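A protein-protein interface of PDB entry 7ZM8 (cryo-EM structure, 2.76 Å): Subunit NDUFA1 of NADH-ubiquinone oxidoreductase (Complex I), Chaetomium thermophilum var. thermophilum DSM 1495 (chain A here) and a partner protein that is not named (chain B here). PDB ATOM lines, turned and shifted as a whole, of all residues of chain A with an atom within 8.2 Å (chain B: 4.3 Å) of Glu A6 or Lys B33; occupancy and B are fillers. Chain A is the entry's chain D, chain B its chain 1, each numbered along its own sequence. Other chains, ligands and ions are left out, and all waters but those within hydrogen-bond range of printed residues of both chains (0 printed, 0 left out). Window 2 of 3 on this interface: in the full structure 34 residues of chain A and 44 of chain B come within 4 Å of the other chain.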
ATOM      1  N   PRO A   2      14.252  21.964  32.348  1.00  0.00           N
ATOM      2  CA  PRO A   2      13.191  21.028  32.723  1.00  0.00           C
ATOM      3  C   PRO A   2      12.973  19.946  31.676  1.00  0.00           C
ATOM      4  O   PRO A   2      13.462  20.062  30.556  1.00  0.00           O
ATOM      5  CB  PRO A   2      11.949  21.923  32.839  1.00  0.00           C
ATOM      6  CG  PRO A   2      12.433  23.326  32.689  1.00  0.00           C
ATOM      7  CD  PRO A   2      13.705  23.262  31.931  1.00  0.00           C
ATOM      8  N   VAL A   3      12.232  18.909  32.044  1.00  0.00           N
ATOM      9  CA  VAL A   3      11.912  17.811  31.139  1.00  0.00           C
ATOM     10  C   VAL A   3      10.685  18.213  30.327  1.00  0.00           C
ATOM     11  O   VAL A   3       9.636  18.498  30.920  1.00  0.00           O
ATOM     12  CB  VAL A   3      11.655  16.511  31.905  1.00  0.00           C
ATOM     13  CG1 VAL A   3      11.313  15.393  30.945  1.00  0.00           C
ATOM     14  CG2 VAL A   3      12.858  16.159  32.744  1.00  0.00           C
ATOM     15  N   PRO A   4      10.770  18.261  29.008  1.00  0.00           N
ATOM     16  CA  PRO A   4       9.578  18.535  28.191  1.00  0.00           C
ATOM     17  C   PRO A   4       8.791  17.258  27.910  1.00  0.00           C
ATOM     18  O   PRO A   4       8.896  16.626  26.863  1.00  0.00           O
ATOM     19  CB  PRO A   4      10.178  19.142  26.921  1.00  0.00           C
ATOM     20  CG  PRO A   4      11.514  18.512  26.805  1.00  0.00           C
ATOM     21  CD  PRO A   4      11.991  18.176  28.190  1.00  0.00           C
ATOM     22  N   PHE A   5       7.978  16.855  28.889  1.00  0.00           N
ATOM     23  CA  PHE A   5       7.295  15.568  28.799  1.00  0.00           C
ATOM     24  C   PHE A   5       6.338  15.504  27.617  1.00  0.00           C
ATOM     25  O   PHE A   5       6.061  14.417  27.103  1.00  0.00           O
ATOM     26  CB  PHE A   5       6.548  15.276  30.102  1.00  0.00           C
ATOM     27  CG  PHE A   5       5.335  16.137  30.312  1.00  0.00           C
ATOM     28  CD1 PHE A   5       4.099  15.752  29.820  1.00  0.00           C
ATOM     29  CD2 PHE A   5       5.430  17.326  31.001  1.00  0.00           C
ATOM     30  CE1 PHE A   5       2.992  16.537  30.005  1.00  0.00           C
ATOM     31  CE2 PHE A   5       4.322  18.111  31.195  1.00  0.00           C
ATOM     32  CZ  PHE A   5       3.103  17.718  30.698  1.00  0.00           C
ATOM     33  N   GLU A   6       5.817  16.648  27.177  1.00  0.00           N
ATOM     34  CA  GLU A   6       4.857  16.640  26.079  1.00  0.00           C
ATOM     35  C   GLU A   6       5.491  16.153  24.786  1.00  0.00           C
ATOM     36  O   GLU A   6       4.805  15.568  23.943  1.00  0.00           O
ATOM     37  CB  GLU A   6       4.252  18.032  25.894  1.00  0.00           C
ATOM     38  CG  GLU A   6       5.213  19.069  25.326  1.00  0.00           C
ATOM     39  CD  GLU A   6       6.280  19.495  26.321  1.00  0.00           C
ATOM     40  OE1 GLU A   6       6.085  19.283  27.538  1.00  0.00           O
ATOM     41  OE2 GLU A   6       7.321  20.023  25.879  1.00  0.00           O
ATOM     42  N   THR A   7       6.789  16.379  24.609  1.00  0.00           N
ATOM     43  CA  THR A   7       7.489  15.820  23.464  1.00  0.00           C
ATOM     44  C   THR A   7       7.790  14.344  23.647  1.00  0.00           C
ATOM     45  O   THR A   7       8.006  13.640  22.656  1.00  0.00           O
ATOM     46  CB  THR A   7       8.789  16.581  23.206  1.00  0.00           C
ATOM     47  OG1 THR A   7       9.797  16.132  24.113  1.00  0.00           O
ATOM     48  CG2 THR A   7       8.567  18.068  23.408  1.00  0.00           C
ATOM     49  N   LEU A   8       7.803  13.866  24.889  1.00  0.00           N
ATOM     50  CA  LEU A   8       8.034  12.458  25.169  1.00  0.00           C
ATOM     51  C   LEU A   8       6.783  11.615  24.995  1.00  0.00           C
ATOM     52  O   LEU A   8       6.886  10.390  24.910  1.00  0.00           O
ATOM     53  CB  LEU A   8       8.563  12.280  26.592  1.00  0.00           C
ATOM     54  CG  LEU A   8      10.056  12.478  26.844  1.00  0.00           C
ATOM     55  CD1 LEU A   8      10.859  11.430  26.086  1.00  0.00           C
ATOM     56  CD2 LEU A   8      10.520  13.879  26.500  1.00  0.00           C
ATOM     57  N   ILE A   9       5.609  12.241  24.953  1.00  0.00           N
ATOM     58  CA  ILE A   9       4.365  11.483  24.825  1.00  0.00           C
ATOM     59  C   ILE A   9       4.317  10.664  23.542  1.00  0.00           C
ATOM     60  O   ILE A   9       3.925   9.487  23.605  1.00  0.00           O
ATOM     61  CB  ILE A   9       3.156  12.421  24.986  1.00  0.00           C
ATOM     62  CG1 ILE A   9       2.939  12.748  26.462  1.00  0.00           C
ATOM     63  CG2 ILE A   9       1.911  11.808  24.376  1.00  0.00           C
ATOM     64  CD1 ILE A   9       2.355  14.111  26.708  1.00  0.00           C
ATOM     65  N   PRO A  10       4.672  11.197  22.366  1.00  0.00           N
ATOM     66  CA  PRO A  10       4.691  10.328  21.179  1.00  0.00           C
ATOM     67  C   PRO A  10       5.603   9.127  21.331  1.00  0.00           C
ATOM     68  O   PRO A  10       5.282   8.048  20.825  1.00  0.00           O
ATOM     69  CB  PRO A  10       5.173  11.271  20.071  1.00  0.00           C
ATOM     70  CG  PRO A  10       4.753  12.594  20.515  1.00  0.00           C
ATOM     71  CD  PRO A  10       4.917  12.602  21.997  1.00  0.00           C
ATOM     72  N   TYR A  11       6.737   9.290  22.015  1.00  0.00           N
ATOM     73  CA  TYR A  11       7.679   8.188  22.171  1.00  0.00           C
ATOM     74  C   TYR A  11       7.088   7.070  23.016  1.00  0.00           C
ATOM     75  O   TYR A  11       7.343   5.891  22.757  1.00  0.00           O
ATOM     76  CB  TYR A  11       8.980   8.699  22.782  1.00  0.00           C
ATOM     77  CG  TYR A  11       9.855   9.429  21.796  1.00  0.00           C
ATOM     78  CD1 TYR A  11      10.699   8.735  20.945  1.00  0.00           C
ATOM     79  CD2 TYR A  11       9.830  10.811  21.709  1.00  0.00           C
ATOM     80  CE1 TYR A  11      11.502   9.398  20.037  1.00  0.00           C
ATOM     81  CE2 TYR A  11      10.629  11.484  20.805  1.00  0.00           C
ATOM     82  CZ  TYR A  11      11.460  10.771  19.973  1.00  0.00           C
ATOM     83  OH  TYR A  11      12.256  11.435  19.076  1.00  0.00           O
ATOM     84  N   ILE A  13       3.954   6.279  23.057  1.00  0.00           N
ATOM     85  CA  ILE A  13       2.971   5.597  22.223  1.00  0.00           C
ATOM     86  C   ILE A  13       3.643   4.525  21.376  1.00  0.00           C
ATOM     87  O   ILE A  13       3.108   3.425  21.201  1.00  0.00           O
ATOM     88  CB  ILE A  13       2.209   6.614  21.356  1.00  0.00           C
ATOM     89  CG1 ILE A  13       1.474   7.619  22.239  1.00  0.00           C
ATOM     90  CG2 ILE A  13       1.229   5.916  20.450  1.00  0.00           C
ATOM     91  CD1 ILE A  13       1.168   8.916  21.553  1.00  0.00           C
ATOM     92  N   VAL B  29       4.903  13.060  14.345  1.00  0.00           N
ATOM     93  CA  VAL B  29       4.607  14.052  15.412  1.00  0.00           C
ATOM     94  C   VAL B  29       5.847  14.185  16.286  1.00  0.00           C
ATOM     95  O   VAL B  29       6.188  15.308  16.644  1.00  0.00           O
ATOM     96  CB  VAL B  29       3.379  13.605  16.227  1.00  0.00           C
ATOM     97  CG1 VAL B  29       3.088  14.528  17.401  1.00  0.00           C
ATOM     98  CG2 VAL B  29       2.149  13.449  15.352  1.00  0.00           C
ATOM     99  N   GLY B  30       6.495  13.071  16.592  1.00  0.00           N
ATOM    100  CA  GLY B  30       7.692  13.062  17.449  1.00  0.00           C
ATOM    101  C   GLY B  30       8.874  13.791  16.850  1.00  0.00           C
ATOM    102  O   GLY B  30       9.608  14.418  17.600  1.00  0.00           O
ATOM    103  N   GLU B  31       9.061  13.693  15.538  1.00  0.00           N
ATOM    104  CA  GLU B  31      10.154  14.442  14.879  1.00  0.00           C
ATOM    105  C   GLU B  31       9.937  15.922  15.160  1.00  0.00           C
ATOM    106  O   GLU B  31      10.887  16.579  15.605  1.00  0.00           O
ATOM    107  CB  GLU B  31      10.168  14.170  13.375  1.00  0.00           C
ATOM    108  CG  GLU B  31      11.487  14.541  12.723  1.00  0.00           C
ATOM    109  CD  GLU B  31      11.416  14.823  11.235  1.00  0.00           C
ATOM    110  OE1 GLU B  31      12.392  14.506  10.531  1.00  0.00           O
ATOM    111  OE2 GLU B  31      10.390  15.374  10.787  1.00  0.00           O
ATOM    112  N   ARG B  32       8.727  16.418  14.915  1.00  0.00           N
ATOM    113  CA  ARG B  32       8.453  17.865  15.080  1.00  0.00           C
ATOM    114  C   ARG B  32       8.609  18.257  16.554  1.00  0.00           C
ATOM    115  O   ARG B  32       9.239  19.289  16.816  1.00  0.00           O
ATOM    116  CB  ARG B  32       7.090  18.171  14.456  1.00  0.00           C
ATOM    117  CG  ARG B  32       6.940  17.659  13.031  1.00  0.00           C
ATOM    118  CD  ARG B  32       5.536  17.834  12.488  1.00  0.00           C
ATOM    119  NE  ARG B  32       5.203  19.233  12.280  1.00  0.00           N
ATOM    120  CZ  ARG B  32       4.029  19.670  11.840  1.00  0.00           C
ATOM    121  NH1 ARG B  32       3.067  18.809  11.560  1.00  0.00           N
ATOM    122  NH2 ARG B  32       3.823  20.965  11.685  1.00  0.00           N
ATOM    123  N   LYS B  33       8.068  17.457  17.473  1.00  0.00           N
ATOM    124  CA  LYS B  33       8.125  17.773  18.924  1.00  0.00           C
ATOM    125  C   LYS B  33       9.569  17.752  19.440  1.00  0.00           C
ATOM    126  O   LYS B  33       9.898  18.602  20.277  1.00  0.00           O
ATOM    127  CB  LYS B  33       7.120  16.926  19.710  1.00  0.00           C
ATOM    128  CG  LYS B  33       5.659  17.212  19.394  1.00  0.00           C
ATOM    129  CD  LYS B  33       4.738  17.062  20.581  1.00  0.00           C
ATOM    130  CE  LYS B  33       4.975  18.106  21.652  1.00  0.00           C
ATOM    131  NZ  LYS B  33       4.472  19.445  21.265  1.00  0.00           N
ATOM    132  N   THR B  34      10.388  16.814  18.968  1.00  0.00           N
ATOM    133  CA  THR B  34      11.808  16.723  19.393  1.00  0.00           C
ATOM    134  C   THR B  34      12.610  17.908  18.840  1.00  0.00           C
ATOM    135  O   THR B  34      13.304  18.554  19.636  1.00  0.00           O
ATOM    136  CB  THR B  34      12.386  15.370  18.969  1.00  0.00           C
ATOM    137  OG1 THR B  34      11.498  14.368  19.460  1.00  0.00           O
ATOM    138  CG2 THR B  34      13.777  15.121  19.507  1.00  0.00           C
ATOM    139  N   MET B  35      12.515  18.176  17.537  1.00  0.00           N
ATOM    140  CA  MET B  35      13.264  19.283  16.880  1.00  0.00           C
ATOM    141  C   MET B  35      12.936  20.585  17.592  1.00  0.00           C
ATOM    142  O   MET B  35      13.842  21.384  17.749  1.00  0.00           O
ATOM    143  CB  MET B  35      12.856  19.433  15.416  1.00  0.00           C
ATOM    144  CG  MET B  35      13.239  18.261  14.563  1.00  0.00           C
ATOM    145  SD  MET B  35      14.602  18.585  13.442  1.00  0.00           S
ATOM    146  CE  MET B  35      14.791  16.936  12.776  1.00  0.00           C
ATOM    147  N   GLY B  36      11.697  20.744  18.046  1.00  0.00           N
ATOM    148  CA  GLY B  36      11.264  21.961  18.741  1.00  0.00           C
ATOM    149  C   GLY B  36      11.881  22.053  20.117  1.00  0.00           C
ATOM    150  O   GLY B  36      12.360  23.132  20.415  1.00  0.00           O
ATOM    151  N   SER B  37      11.960  20.979  20.904  1.00  0.00           N
ATOM    152  CA  SER B  37      12.660  21.099  22.181  1.00  0.00           C
ATOM    153  C   SER B  37      14.118  21.487  21.987  1.00  0.00           C
ATOM    154  O   SER B  37      14.632  22.353  22.700  1.00  0.00           O
ATOM    155  CB  SER B  37      12.567  19.797  22.969  1.00  0.00           C
ATOM    156  OG  SER B  37      11.280  19.629  23.512  1.00  0.00           O
ATOM    157  N   GLY B  43       6.686  21.631  19.696  1.00  0.00           N
ATOM    158  CA  GLY B  43       6.197  20.928  18.537  1.00  0.00           C
ATOM    159  C   GLY B  43       4.729  21.228  18.324  1.00  0.00           C
ATOM    160  O   GLY B  43       4.205  22.231  18.809  1.00  0.00           O
ATOM    161  N   PRO B  44       4.038  20.371  17.583  1.00  0.00           N
ATOM    162  CA  PRO B  44       2.581  20.491  17.496  1.00  0.00           C
ATOM    163  C   PRO B  44       1.927  20.311  18.859  1.00  0.00           C
ATOM    164  O   PRO B  44       2.220  19.364  19.589  1.00  0.00           O
ATOM    165  CB  PRO B  44       2.195  19.370  16.527  1.00  0.00           C
ATOM    166  CG  PRO B  44       3.406  19.176  15.690  1.00  0.00           C
ATOM    167  CD  PRO B  44       4.573  19.425  16.592  1.00  0.00           C
ATOM    168  N   TYR B  50      -2.779  17.234  23.061  1.00  0.00           N
ATOM    169  CA  TYR B  50      -1.365  17.572  23.162  1.00  0.00           C
ATOM    170  C   TYR B  50      -0.701  17.525  21.796  1.00  0.00           C
ATOM    171  O   TYR B  50       0.477  17.186  21.681  1.00  0.00           O
ATOM    172  CB  TYR B  50      -0.654  16.639  24.140  1.00  0.00           C
ATOM    173  CG  TYR B  50      -0.607  17.149  25.562  1.00  0.00           C
ATOM    174  CD1 TYR B  50       0.101  18.296  25.887  1.00  0.00           C
ATOM    175  CD2 TYR B  50      -1.265  16.479  26.579  1.00  0.00           C
ATOM    176  CE1 TYR B  50       0.151  18.759  27.179  1.00  0.00           C
ATOM    177  CE2 TYR B  50      -1.220  16.935  27.873  1.00  0.00           C
ATOM    178  CZ  TYR B  50      -0.510  18.076  28.171  1.00  0.00           C
ATOM    179  OH  TYR B  50      -0.467  18.536  29.467  1.00  0.00           O
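The side-chain hydroxyl of Thr B34 sits at hydrogen-bond distance from the side-chain hydroxyl of Tyr A11 (3.1 Å).
The side-chain amino group (NZ) of Lys B33 sits at hydrogen-bond distance from the backbone carbonyl oxygen (O) of Pro B44, 2.8 Å away. The backbone carbonyl oxygen of Gly B30 sits at hydrogen-bond distance from the side-chain hydroxyl of Thr B34 (2.7 Å). O of Pro A4 is in hydrogen-bond range of OG1 of Thr A7, 2.9 Å away.
Ser B37 touches Pro A4. Phe A5 touches Tyr B50. CE of Lys B33 touches O of Glu A6, at 3.4 Å. O of Lys B33 touches CG2 of Thr A7, 3.4 Å away. Ser B37 touches Thr A7.
Printed residues of chain B within 4 Å of Pro A4: Ser B37. Of the printed residues of chain B, Phe A5 touches Tyr B50. Of chain A, only Glu A6 and Thr A7 come within 4 Å of Lys B33. Of the printed residues of chain A, Ser B37 touches Pro A4 (3.5 Å) and Thr A7 (3.1 Å). No residue of chain A comes within 4 Å of Gly B43. The nearest residue of chain A that does not touch Lys B33 is Pro A10 (4.5 Å).
Hydrophobic or aromatic side chains of chain A within 4 Å of the printed part of chain B: Pro A4, Phe A5 and Tyr A11. Along chain A the printed residues that touch a printed residue of chain B span positions 4 to 11. Of the 12 printed residues of chain B, 4 touch a printed residue of chain A. Hydrophobic or aromatic side chains of chain B that line the printed part of chain A: Tyr B50. Among the printed residues, no Asp or Glu carboxylate lies within 4 Å of a Lys or Arg side-chain nitrogen of the other chain.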
